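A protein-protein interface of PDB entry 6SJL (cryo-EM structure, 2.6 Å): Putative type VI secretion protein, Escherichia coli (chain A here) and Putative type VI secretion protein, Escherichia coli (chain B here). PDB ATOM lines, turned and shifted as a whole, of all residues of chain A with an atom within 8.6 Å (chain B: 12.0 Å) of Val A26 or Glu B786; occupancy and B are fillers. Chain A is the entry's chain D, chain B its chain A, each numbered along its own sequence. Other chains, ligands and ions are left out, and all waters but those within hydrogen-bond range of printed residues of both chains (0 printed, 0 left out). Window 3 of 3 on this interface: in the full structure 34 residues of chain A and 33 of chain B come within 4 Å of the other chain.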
ATOM      1  N   TYR A   7      -4.619 -26.565  25.522  1.00  0.00           N
ATOM      2  CA  TYR A   7      -5.796 -26.759  24.684  1.00  0.00           C
ATOM      3  C   TYR A   7      -6.077 -25.486  23.906  1.00  0.00           C
ATOM      4  O   TYR A   7      -6.591 -24.512  24.468  1.00  0.00           O
ATOM      5  CB  TYR A   7      -7.012 -27.139  25.527  1.00  0.00           C
ATOM      6  CG  TYR A   7      -6.764 -28.311  26.433  1.00  0.00           C
ATOM      7  CD1 TYR A   7      -6.619 -29.587  25.923  1.00  0.00           C
ATOM      8  CD2 TYR A   7      -6.676 -28.139  27.802  1.00  0.00           C
ATOM      9  CE1 TYR A   7      -6.386 -30.659  26.750  1.00  0.00           C
ATOM     10  CE2 TYR A   7      -6.448 -29.204  28.635  1.00  0.00           C
ATOM     11  CZ  TYR A   7      -6.301 -30.465  28.104  1.00  0.00           C
ATOM     12  OH  TYR A   7      -6.072 -31.538  28.929  1.00  0.00           O
ATOM     13  N   ASP A   8      -5.772 -25.509  22.611  1.00  0.00           N
ATOM     14  CA  ASP A   8      -6.060 -24.386  21.722  1.00  0.00           C
ATOM     15  C   ASP A   8      -7.565 -24.364  21.518  1.00  0.00           C
ATOM     16  O   ASP A   8      -8.104 -25.010  20.620  1.00  0.00           O
ATOM     17  CB  ASP A   8      -5.324 -24.537  20.400  1.00  0.00           C
ATOM     18  CG  ASP A   8      -3.825 -24.514  20.567  1.00  0.00           C
ATOM     19  OD1 ASP A   8      -3.342 -23.891  21.532  1.00  0.00           O
ATOM     20  OD2 ASP A   8      -3.131 -25.116  19.727  1.00  0.00           O
ATOM     21  N   VAL A   9      -8.254 -23.633  22.378  1.00  0.00           N
ATOM     22  CA  VAL A   9      -9.707 -23.646  22.403  1.00  0.00           C
ATOM     23  C   VAL A   9     -10.223 -22.386  21.725  1.00  0.00           C
ATOM     24  O   VAL A   9      -9.593 -21.321  21.783  1.00  0.00           O
ATOM     25  CB  VAL A   9     -10.245 -23.773  23.843  1.00  0.00           C
ATOM     26  CG1 VAL A   9     -10.111 -22.463  24.600  1.00  0.00           C
ATOM     27  CG2 VAL A   9     -11.681 -24.253  23.845  1.00  0.00           C
ATOM     28  N   THR A  10     -11.353 -22.529  21.037  1.00  0.00           N
ATOM     29  CA  THR A  10     -12.131 -21.403  20.548  1.00  0.00           C
ATOM     30  C   THR A  10     -13.546 -21.402  21.090  1.00  0.00           C
ATOM     31  O   THR A  10     -14.221 -20.367  21.006  1.00  0.00           O
ATOM     32  CB  THR A  10     -12.188 -21.401  19.012  1.00  0.00           C
ATOM     33  OG1 THR A  10     -12.897 -22.555  18.555  1.00  0.00           O
ATOM     34  CG2 THR A  10     -10.788 -21.433  18.432  1.00  0.00           C
ATOM     35  N   ASP A  11     -14.018 -22.519  21.640  1.00  0.00           N
ATOM     36  CA  ASP A  11     -15.315 -22.593  22.304  1.00  0.00           C
ATOM     37  C   ASP A  11     -15.192 -22.053  23.731  1.00  0.00           C
ATOM     38  O   ASP A  11     -15.479 -22.720  24.726  1.00  0.00           O
ATOM     39  CB  ASP A  11     -15.808 -24.030  22.278  1.00  0.00           C
ATOM     40  CG  ASP A  11     -15.515 -24.709  20.958  1.00  0.00           C
ATOM     41  OD1 ASP A  11     -15.680 -24.066  19.902  1.00  0.00           O
ATOM     42  OD2 ASP A  11     -15.103 -25.882  20.974  1.00  0.00           O
ATOM     43  N   ALA A  12     -14.741 -20.803  23.805  1.00  0.00           N
ATOM     44  CA  ALA A  12     -14.356 -20.169  25.054  1.00  0.00           C
ATOM     45  C   ALA A  12     -15.332 -19.082  25.472  1.00  0.00           C
ATOM     46  O   ALA A  12     -14.959 -18.187  26.236  1.00  0.00           O
ATOM     47  CB  ALA A  12     -12.944 -19.594  24.932  1.00  0.00           C
ATOM     48  N   LYS A  23     -21.833 -25.398  28.919  1.00  0.00           N
ATOM     49  CA  LYS A  23     -21.804 -25.240  27.467  1.00  0.00           C
ATOM     50  C   LYS A  23     -20.994 -26.316  26.746  1.00  0.00           C
ATOM     51  O   LYS A  23     -21.560 -27.340  26.358  1.00  0.00           O
ATOM     52  CB  LYS A  23     -21.234 -23.849  27.140  1.00  0.00           C
ATOM     53  CG  LYS A  23     -20.965 -23.553  25.666  1.00  0.00           C
ATOM     54  CD  LYS A  23     -22.208 -23.420  24.818  1.00  0.00           C
ATOM     55  CE  LYS A  23     -22.901 -22.104  25.076  1.00  0.00           C
ATOM     56  NZ  LYS A  23     -22.052 -20.960  24.633  1.00  0.00           N
ATOM     57  N   VAL A  24     -19.672 -26.141  26.658  1.00  0.00           N
ATOM     58  CA  VAL A  24     -18.700 -27.058  26.051  1.00  0.00           C
ATOM     59  C   VAL A  24     -17.299 -26.517  26.301  1.00  0.00           C
ATOM     60  O   VAL A  24     -17.114 -25.307  26.450  1.00  0.00           O
ATOM     61  CB  VAL A  24     -18.884 -27.258  24.529  1.00  0.00           C
ATOM     62  CG1 VAL A  24     -19.991 -28.234  24.178  1.00  0.00           C
ATOM     63  CG2 VAL A  24     -19.103 -25.921  23.845  1.00  0.00           C
ATOM     64  N   VAL A  25     -16.301 -27.395  26.310  1.00  0.00           N
ATOM     65  CA  VAL A  25     -14.957 -26.988  25.913  1.00  0.00           C
ATOM     66  C   VAL A  25     -14.420 -28.055  24.970  1.00  0.00           C
ATOM     67  O   VAL A  25     -13.939 -29.106  25.409  1.00  0.00           O
ATOM     68  CB  VAL A  25     -14.003 -26.776  27.105  1.00  0.00           C
ATOM     69  CG1 VAL A  25     -12.610 -26.441  26.604  1.00  0.00           C
ATOM     70  CG2 VAL A  25     -14.487 -25.672  28.006  1.00  0.00           C
ATOM     71  N   VAL A  26     -14.521 -27.805  23.668  1.00  0.00           N
ATOM     72  CA  VAL A  26     -13.964 -28.691  22.656  1.00  0.00           C
ATOM     73  C   VAL A  26     -12.646 -28.094  22.192  1.00  0.00           C
ATOM     74  O   VAL A  26     -12.618 -27.003  21.610  1.00  0.00           O
ATOM     75  CB  VAL A  26     -14.938 -28.897  21.487  1.00  0.00           C
ATOM     76  CG1 VAL A  26     -14.266 -29.662  20.357  1.00  0.00           C
ATOM     77  CG2 VAL A  26     -16.182 -29.623  21.974  1.00  0.00           C
ATOM     78  N   ALA A  27     -11.553 -28.803  22.466  1.00  0.00           N
ATOM     79  CA  ALA A  27     -10.216 -28.323  22.153  1.00  0.00           C
ATOM     80  C   ALA A  27      -9.294 -29.518  21.991  1.00  0.00           C
ATOM     81  O   ALA A  27      -9.367 -30.468  22.774  1.00  0.00           O
ATOM     82  CB  ALA A  27      -9.699 -27.388  23.245  1.00  0.00           C
ATOM     83  N   LYS A  28      -8.441 -29.469  20.973  1.00  0.00           N
ATOM     84  CA  LYS A  28      -7.543 -30.569  20.657  1.00  0.00           C
ATOM     85  C   LYS A  28      -6.259 -30.473  21.481  1.00  0.00           C
ATOM     86  O   LYS A  28      -5.854 -29.393  21.919  1.00  0.00           O
ATOM     87  CB  LYS A  28      -7.237 -30.562  19.161  1.00  0.00           C
ATOM     88  CG  LYS A  28      -6.590 -31.817  18.612  1.00  0.00           C
ATOM     89  CD  LYS A  28      -5.083 -31.701  18.495  1.00  0.00           C
ATOM     90  CE  LYS A  28      -4.533 -32.931  17.792  1.00  0.00           C
ATOM     91  NZ  LYS A  28      -3.059 -32.924  17.650  1.00  0.00           N
ATOM     92  N   LYS A  29      -5.623 -31.626  21.697  1.00  0.00           N
ATOM     93  CA  LYS A  29      -4.405 -31.692  22.497  1.00  0.00           C
ATOM     94  C   LYS A  29      -3.269 -30.964  21.794  1.00  0.00           C
ATOM     95  O   LYS A  29      -2.737 -31.453  20.793  1.00  0.00           O
ATOM     96  CB  LYS A  29      -4.004 -33.146  22.737  1.00  0.00           C
ATOM     97  CG  LYS A  29      -5.065 -33.980  23.400  1.00  0.00           C
ATOM     98  CD  LYS A  29      -5.299 -33.527  24.817  1.00  0.00           C
ATOM     99  CE  LYS A  29      -6.387 -34.340  25.457  1.00  0.00           C
ATOM    100  NZ  LYS A  29      -5.988 -35.754  25.648  1.00  0.00           N
ATOM    101  N   GLY B 780     -21.504 -23.711  33.571  1.00  0.00           N
ATOM    102  CA  GLY B 780     -20.092 -24.030  33.492  1.00  0.00           C
ATOM    103  C   GLY B 780     -19.716 -24.601  32.147  1.00  0.00           C
ATOM    104  O   GLY B 780     -20.297 -24.246  31.120  1.00  0.00           O
ATOM    105  N   PHE B 781     -18.713 -25.480  32.154  1.00  0.00           N
ATOM    106  CA  PHE B 781     -18.142 -26.043  30.937  1.00  0.00           C
ATOM    107  C   PHE B 781     -17.773 -27.502  31.169  1.00  0.00           C
ATOM    108  O   PHE B 781     -17.634 -27.959  32.308  1.00  0.00           O
ATOM    109  CB  PHE B 781     -16.896 -25.270  30.488  1.00  0.00           C
ATOM    110  CG  PHE B 781     -17.151 -23.835  30.099  1.00  0.00           C
ATOM    111  CD1 PHE B 781     -17.316 -22.850  31.059  1.00  0.00           C
ATOM    112  CD2 PHE B 781     -17.171 -23.464  28.767  1.00  0.00           C
ATOM    113  CE1 PHE B 781     -17.533 -21.535  30.696  1.00  0.00           C
ATOM    114  CE2 PHE B 781     -17.382 -22.151  28.400  1.00  0.00           C
ATOM    115  CZ  PHE B 781     -17.561 -21.185  29.370  1.00  0.00           C
ATOM    116  N   ILE B 782     -17.605 -28.238  30.069  1.00  0.00           N
ATOM    117  CA  ILE B 782     -16.993 -29.563  30.082  1.00  0.00           C
ATOM    118  C   ILE B 782     -15.883 -29.560  29.046  1.00  0.00           C
ATOM    119  O   ILE B 782     -16.143 -29.346  27.856  1.00  0.00           O
ATOM    120  CB  ILE B 782     -17.974 -30.712  29.777  1.00  0.00           C
ATOM    121  CG1 ILE B 782     -19.087 -30.826  30.817  1.00  0.00           C
ATOM    122  CG2 ILE B 782     -17.224 -32.031  29.685  1.00  0.00           C
ATOM    123  CD1 ILE B 782     -20.393 -30.284  30.347  1.00  0.00           C
ATOM    124  N   LEU B 783     -14.655 -29.806  29.487  1.00  0.00           N
ATOM    125  CA  LEU B 783     -13.530 -29.842  28.561  1.00  0.00           C
ATOM    126  C   LEU B 783     -13.522 -31.218  27.916  1.00  0.00           C
ATOM    127  O   LEU B 783     -13.193 -32.212  28.560  1.00  0.00           O
ATOM    128  CB  LEU B 783     -12.214 -29.570  29.277  1.00  0.00           C
ATOM    129  CG  LEU B 783     -11.101 -28.955  28.413  1.00  0.00           C
ATOM    130  CD1 LEU B 783      -9.967 -28.435  29.272  1.00  0.00           C
ATOM    131  CD2 LEU B 783     -10.593 -29.798  27.251  1.00  0.00           C
ATOM    132  N   THR B 784     -13.906 -31.294  26.649  1.00  0.00           N
ATOM    133  CA  THR B 784     -13.785 -32.522  25.881  1.00  0.00           C
ATOM    134  C   THR B 784     -12.855 -32.300  24.698  1.00  0.00           C
ATOM    135  O   THR B 784     -12.968 -31.299  23.987  1.00  0.00           O
ATOM    136  CB  THR B 784     -15.152 -33.007  25.396  1.00  0.00           C
ATOM    137  OG1 THR B 784     -15.789 -31.970  24.639  1.00  0.00           O
ATOM    138  CG2 THR B 784     -16.032 -33.390  26.576  1.00  0.00           C
ATOM    139  N   ASP B 785     -11.928 -33.227  24.495  1.00  0.00           N
ATOM    140  CA  ASP B 785     -11.078 -33.141  23.320  1.00  0.00           C
ATOM    141  C   ASP B 785     -11.804 -33.703  22.101  1.00  0.00           C
ATOM    142  O   ASP B 785     -12.915 -34.234  22.194  1.00  0.00           O
ATOM    143  CB  ASP B 785      -9.747 -33.853  23.553  1.00  0.00           C
ATOM    144  CG  ASP B 785      -9.905 -35.332  23.832  1.00  0.00           C
ATOM    145  OD1 ASP B 785      -8.948 -35.929  24.369  1.00  0.00           O
ATOM    146  OD2 ASP B 785     -10.967 -35.907  23.523  1.00  0.00           O
ATOM    147  N   GLU B 786     -11.138 -33.602  20.945  1.00  0.00           N
ATOM    148  CA  GLU B 786     -11.754 -33.940  19.665  1.00  0.00           C
ATOM    149  C   GLU B 786     -12.388 -35.330  19.641  1.00  0.00           C
ATOM    150  O   GLU B 786     -13.285 -35.571  18.827  1.00  0.00           O
ATOM    151  CB  GLU B 786     -10.711 -33.833  18.551  1.00  0.00           C
ATOM    152  CG  GLU B 786     -10.144 -32.434  18.343  1.00  0.00           C
ATOM    153  CD  GLU B 786     -11.095 -31.476  17.641  1.00  0.00           C
ATOM    154  OE1 GLU B 786     -12.185 -31.202  18.187  1.00  0.00           O
ATOM    155  OE2 GLU B 786     -10.747 -30.991  16.544  1.00  0.00           O
ATOM    156  N   ALA B 787     -11.960 -36.242  20.514  1.00  0.00           N
ATOM    157  CA  ALA B 787     -12.538 -37.582  20.560  1.00  0.00           C
ATOM    158  C   ALA B 787     -13.804 -37.638  21.404  1.00  0.00           C
ATOM    159  O   ALA B 787     -14.811 -38.206  20.971  1.00  0.00           O
ATOM    160  CB  ALA B 787     -11.517 -38.584  21.109  1.00  0.00           C
ATOM    161  N   GLY B 788     -13.777 -37.060  22.602  1.00  0.00           N
ATOM    162  CA  GLY B 788     -14.954 -37.020  23.443  1.00  0.00           C
ATOM    163  C   GLY B 788     -14.663 -37.258  24.910  1.00  0.00           C
ATOM    164  O   GLY B 788     -15.549 -37.107  25.755  1.00  0.00           O
ATOM    165  N   VAL B 789     -13.429 -37.620  25.229  1.00  0.00           N
ATOM    166  CA  VAL B 789     -13.069 -37.909  26.618  1.00  0.00           C
ATOM    167  C   VAL B 789     -13.024 -36.596  27.395  1.00  0.00           C
ATOM    168  O   VAL B 789     -12.463 -35.607  26.897  1.00  0.00           O
ATOM    169  CB  VAL B 789     -11.741 -38.655  26.689  1.00  0.00           C
ATOM    170  CG1 VAL B 789     -11.875 -39.995  25.992  1.00  0.00           C
ATOM    171  CG2 VAL B 789     -10.646 -37.876  26.040  1.00  0.00           C
ATOM    172  N   PRO B 790     -13.633 -36.527  28.580  1.00  0.00           N
ATOM    173  CA  PRO B 790     -13.915 -35.219  29.181  1.00  0.00           C
ATOM    174  C   PRO B 790     -12.773 -34.610  29.981  1.00  0.00           C
ATOM    175  O   PRO B 790     -13.024 -34.006  31.026  1.00  0.00           O
ATOM    176  CB  PRO B 790     -15.104 -35.527  30.094  1.00  0.00           C
ATOM    177  CG  PRO B 790     -14.850 -36.931  30.539  1.00  0.00           C
ATOM    178  CD  PRO B 790     -14.102 -37.636  29.428  1.00  0.00           C
ATOM    179  N   GLN B 791     -11.536 -34.721  29.478  1.00  0.00           N
ATOM    180  CA  GLN B 791     -10.344 -34.002  29.928  1.00  0.00           C
ATOM    181  C   GLN B 791     -10.340 -33.693  31.414  1.00  0.00           C
ATOM    182  O   GLN B 791     -10.583 -32.548  31.816  1.00  0.00           O
ATOM    183  CB  GLN B 791     -10.156 -32.720  29.131  1.00  0.00           C
ATOM    184  CG  GLN B 791      -9.742 -33.021  27.729  1.00  0.00           C
ATOM    185  CD  GLN B 791      -8.827 -34.210  27.669  1.00  0.00           C
ATOM    186  OE1 GLN B 791      -7.769 -34.230  28.297  1.00  0.00           O
ATOM    187  NE2 GLN B 791      -9.221 -35.217  26.909  1.00  0.00           N
ATOM    188  N   PRO B 792     -10.090 -34.684  32.252  1.00  0.00           N
ATOM    189  CA  PRO B 792     -10.221 -34.481  33.691  1.00  0.00           C
ATOM    190  C   PRO B 792      -9.106 -33.616  34.248  1.00  0.00           C
ATOM    191  O   PRO B 792      -8.019 -33.509  33.677  1.00  0.00           O
ATOM    192  CB  PRO B 792     -10.122 -35.904  34.242  1.00  0.00           C
ATOM    193  CG  PRO B 792      -9.177 -36.575  33.284  1.00  0.00           C
ATOM    194  CD  PRO B 792      -9.439 -35.964  31.928  1.00  0.00           C
ATOM    195  N   THR B 794      -7.851 -30.780  34.651  1.00  0.00           N
ATOM    196  CA  THR B 794      -6.944 -29.794  34.092  1.00  0.00           C
ATOM    197  C   THR B 794      -7.273 -28.408  34.625  1.00  0.00           C
ATOM    198  O   THR B 794      -8.449 -28.068  34.777  1.00  0.00           O
ATOM    199  CB  THR B 794      -7.014 -29.787  32.565  1.00  0.00           C
ATOM    200  OG1 THR B 794      -6.325 -28.641  32.053  1.00  0.00           O
ATOM    201  CG2 THR B 794      -8.442 -29.777  32.091  1.00  0.00           C
ATOM    202  N   TYR B 796      -8.084 -24.494  35.012  1.00  0.00           N
ATOM    203  CA  TYR B 796      -8.886 -23.590  34.202  1.00  0.00           C
ATOM    204  C   TYR B 796      -9.018 -22.270  34.941  1.00  0.00           C
ATOM    205  O   TYR B 796      -8.731 -22.172  36.135  1.00  0.00           O
ATOM    206  CB  TYR B 796     -10.266 -24.183  33.895  1.00  0.00           C
ATOM    207  CG  TYR B 796     -11.196 -24.272  35.088  1.00  0.00           C
ATOM    208  CD1 TYR B 796     -11.359 -25.463  35.779  1.00  0.00           C
ATOM    209  CD2 TYR B 796     -11.919 -23.167  35.517  1.00  0.00           C
ATOM    210  CE1 TYR B 796     -12.203 -25.543  36.867  1.00  0.00           C
ATOM    211  CE2 TYR B 796     -12.757 -23.237  36.603  1.00  0.00           C
ATOM    212  CZ  TYR B 796     -12.898 -24.429  37.272  1.00  0.00           C
ATOM    213  OH  TYR B 796     -13.741 -24.507  38.353  1.00  0.00           O
ATOM    214  N   THR B 810     -10.495 -28.629  36.413  1.00  0.00           N
ATOM    215  CA  THR B 810     -11.695 -29.314  35.954  1.00  0.00           C
ATOM    216  C   THR B 810     -11.997 -30.526  36.825  1.00  0.00           C
ATOM    217  O   THR B 810     -11.142 -31.036  37.555  1.00  0.00           O
ATOM    218  CB  THR B 810     -11.566 -29.766  34.504  1.00  0.00           C
ATOM    219  OG1 THR B 810     -10.488 -30.698  34.390  1.00  0.00           O
ATOM    220  CG2 THR B 810     -11.348 -28.579  33.594  1.00  0.00           C
ATOM    221  N   ASN B 813     -15.212 -35.877  34.610  1.00  0.00           N
ATOM    222  CA  ASN B 813     -16.110 -35.548  33.505  1.00  0.00           C
ATOM    223  C   ASN B 813     -15.884 -34.100  33.100  1.00  0.00           C
ATOM    224  O   ASN B 813     -16.690 -33.521  32.367  1.00  0.00           O
ATOM    225  CB  ASN B 813     -17.592 -35.764  33.845  1.00  0.00           C
ATOM    226  CG  ASN B 813     -17.921 -37.210  34.168  1.00  0.00           C
ATOM    227  OD1 ASN B 813     -17.103 -37.934  34.736  1.00  0.00           O
ATOM    228  ND2 ASN B 813     -19.135 -37.630  33.831  1.00  0.00           N
ATOM    229  N   GLY B 814     -14.802 -33.506  33.594  1.00  0.00           N
ATOM    230  CA  GLY B 814     -14.366 -32.207  33.119  1.00  0.00           C
ATOM    231  C   GLY B 814     -15.274 -31.061  33.484  1.00  0.00           C
ATOM    232  O   GLY B 814     -15.375 -30.090  32.729  1.00  0.00           O
ATOM    233  N   LYS B 815     -15.939 -31.142  34.629  1.00  0.00           N
ATOM    234  CA  LYS B 815     -16.861 -30.086  34.992  1.00  0.00           C
ATOM    235  C   LYS B 815     -16.102 -28.857  35.480  1.00  0.00           C
ATOM    236  O   LYS B 815     -14.942 -28.924  35.894  1.00  0.00           O
ATOM    237  CB  LYS B 815     -17.839 -30.564  36.068  1.00  0.00           C
ATOM    238  CG  LYS B 815     -18.700 -31.727  35.626  1.00  0.00           C
ATOM    239  CD  LYS B 815     -19.618 -31.317  34.495  1.00  0.00           C
ATOM    240  CE  LYS B 815     -20.503 -32.466  34.051  1.00  0.00           C
ATOM    241  NZ  LYS B 815     -21.519 -32.804  35.081  1.00  0.00           N
ATOM    242  N   THR B 816     -16.789 -27.728  35.427  1.00  0.00           N
ATOM    243  CA  THR B 816     -16.309 -26.459  35.938  1.00  0.00           C
ATOM    244  C   THR B 816     -17.000 -26.174  37.265  1.00  0.00           C
ATOM    245  O   THR B 816     -17.854 -26.936  37.722  1.00  0.00           O
ATOM    246  CB  THR B 816     -16.585 -25.346  34.922  1.00  0.00           C
ATOM    247  OG1 THR B 816     -16.316 -25.835  33.607  1.00  0.00           O
ATOM    248  CG2 THR B 816     -15.685 -24.178  35.152  1.00  0.00           C
ATOM    249  N   VAL B 827     -15.830 -16.455  30.049  1.00  0.00           N
ATOM    250  CA  VAL B 827     -14.758 -16.866  29.150  1.00  0.00           C
ATOM    251  C   VAL B 827     -13.996 -18.026  29.783  1.00  0.00           C
ATOM    252  O   VAL B 827     -14.090 -18.272  30.989  1.00  0.00           O
ATOM    253  CB  VAL B 827     -13.828 -15.674  28.833  1.00  0.00           C
ATOM    254  CG1 VAL B 827     -12.800 -16.020  27.752  1.00  0.00           C
ATOM    255  CG2 VAL B 827     -14.646 -14.468  28.426  1.00  0.00           C
ATOM    256  N   LYS B 828     -13.232 -18.743  28.961  1.00  0.00           N
ATOM    257  CA  LYS B 828     -12.573 -19.967  29.382  1.00  0.00           C
ATOM    258  C   LYS B 828     -11.110 -19.960  28.953  1.00  0.00           C
ATOM    259  O   LYS B 828     -10.792 -19.530  27.841  1.00  0.00           O
ATOM    260  CB  LYS B 828     -13.265 -21.184  28.762  1.00  0.00           C
ATOM    261  CG  LYS B 828     -12.862 -22.468  29.400  1.00  0.00           C
ATOM    262  CD  LYS B 828     -13.418 -22.502  30.797  1.00  0.00           C
ATOM    263  CE  LYS B 828     -12.708 -23.524  31.623  1.00  0.00           C
ATOM    264  NZ  LYS B 828     -13.035 -24.917  31.219  1.00  0.00           N
ATOM    265  N   VAL B 829     -10.225 -20.450  29.835  1.00  0.00           N
ATOM    266  CA  VAL B 829      -8.835 -20.754  29.500  1.00  0.00           C
ATOM    267  C   VAL B 829      -8.380 -21.977  30.286  1.00  0.00           C
ATOM    268  O   VAL B 829      -8.949 -22.319  31.323  1.00  0.00           O
ATOM    269  CB  VAL B 829      -7.879 -19.576  29.776  1.00  0.00           C
ATOM    270  CG1 VAL B 829      -8.086 -18.460  28.774  1.00  0.00           C
ATOM    271  CG2 VAL B 829      -8.098 -19.057  31.175  1.00  0.00           C
ATOM    272  N   GLU B 830      -7.321 -22.625  29.791  1.00  0.00           N
ATOM    273  CA  GLU B 830      -6.787 -23.833  30.414  1.00  0.00           C
ATOM    274  C   GLU B 830      -5.310 -24.022  30.069  1.00  0.00           C
ATOM    275  O   GLU B 830      -4.838 -23.548  29.034  1.00  0.00           O
ATOM    276  CB  GLU B 830      -7.550 -25.087  29.960  1.00  0.00           C
ATOM    277  CG  GLU B 830      -8.877 -25.351  30.639  1.00  0.00           C
ATOM    278  CD  GLU B 830     -10.046 -25.123  29.713  1.00  0.00           C
ATOM    279  OE1 GLU B 830      -9.842 -24.554  28.620  1.00  0.00           O
ATOM    280  OE2 GLU B 830     -11.165 -25.552  30.057  1.00  0.00           O
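N of Gln B791 sits close to O of Leu B783 (3.1 Å).
The backbone NH (N) of Leu B783 is in hydrogen-bond range of the backbone carbonyl oxygen (O) of Gly B814.
The side-chain carboxylate of Asp B785 lies close to the backbone NH of Ala B787 (3.2 Å).
The backbone NH (N) of Gly B788 is in hydrogen-bond range of the side-chain carboxylate (OD2) of Asp B785, at 3.2 Å.
O of Gln B791 sits at hydrogen-bond distance from OG1 of Thr B810, 3.2 Å away.
The backbone NH (N) of Thr B794 is in hydrogen-bond range of the side-chain hydroxyl (OG1) of Thr B810 (2.7 Å).
O of Gly B780 sits at hydrogen-bond distance from N of Lys A23 (2.9 Å).
The backbone carbonyl oxygen (O) of Ile B782 is in hydrogen-bond range of the backbone NH (N) of Val A25 (2.5 Å).
The backbone NH of Thr B784 sits at hydrogen-bond distance from the backbone carbonyl oxygen of Val A25.
N of Ala A27 is in hydrogen-bond range of O of Thr B784.
NZ of Lys A29 lies within salt-bridge range of OD1 of Asp B785, at 3.2 Å.
OE1 of Gln B791 sits at hydrogen-bond distance from OH of Tyr A7 (3.2 Å).
N of Lys B828 is in hydrogen-bond range of O of Ala A12.
Printed residues of chain B within 4 Å of Tyr A7: Leu B783 (3.6 Å), Gln B791 (3.2 Å), Thr B794 (3.5 Å) and Glu B830 (3.8 Å).
No residue of chain B comes within 4 Å of Val A9.
No residue of chain B comes within 4 Å of Thr A10.
No residue of chain B comes within 4 Å of Asp A11.
Printed residues of chain B within 4 Å of Ala A12: Val B827 and Lys B828.
Of chain B, only Phe B781 (3.0 Å) and Ile B782 (3.4 Å) come within 4 Å of Val A24.
Val A25 touches six residues of chain B.
Of the printed residues of chain B, Lys A28 touches Glu B786 (3.6 Å).
Lys A29 touches just these residues of chain B: Asp B785 and Gln B791.
Printed residues of chain A within 4 Å of Leu B783: Tyr A7 and Val A25.
Glu B786 touches just these residues of chain A: Val A26 (3.4 Å) and Lys A28 (3.6 Å).
Pro B790 touches none of the printed residues of chain A.
Of the printed residues of chain A, Lys B828 touches Ala A12 and Val A25.
The nearest residue of chain B that does not touch Val A26 is Ile B782 (4.7 Å).
The nearest printed residue of chain B that does not touch Ala A12 is Phe B781 (4.7 Å).
Of the 13 printed residues of chain A, 9 touch a printed residue of chain B.
Along chain A the printed residues that touch a printed residue of chain B span positions 7 to 29.
Hydrophobic or aromatic side chains of chain B that line the printed part of chain A: Phe B781, Leu B783 and Val B827.
Along chain B the printed residues that touch a printed residue of chain A span positions 780 to 830.
Among the printed residues, Asp or Glu carboxylates within 4 Å of a Lys or Arg side-chain nitrogen of the other chain: Lys A29 with Asp B785 (3.2 Å).
Among the printed residues, pairs that only touch across the chains: Tyr A7 with Leu B783 (3.6 Å), Tyr A7 with Thr B794 (3.5 Å), Tyr A7 with Glu B830 (3.8 Å), Ala A12 with Val B827 (3.2 Å), Val A24 with Phe B781 (3.0 Å), Val A24 with Ile B782 (3.4 Å), Val A25 with Phe B781 (3.5 Å), Val A25 with Leu B783 (3.3 Å), Val A25 with Lys B828 (3.6 Å), Val A25 with Glu B830 (3.8 Å), Val A26 with Thr B784 (3.1 Å), Val A26 with Glu B786 (3.4 Å), Ala A27 with Asp B785 (3.2 Å), Lys A28 with Glu B786 (3.6 Å) and Lys A29 with Gln B791 (3.2 Å).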
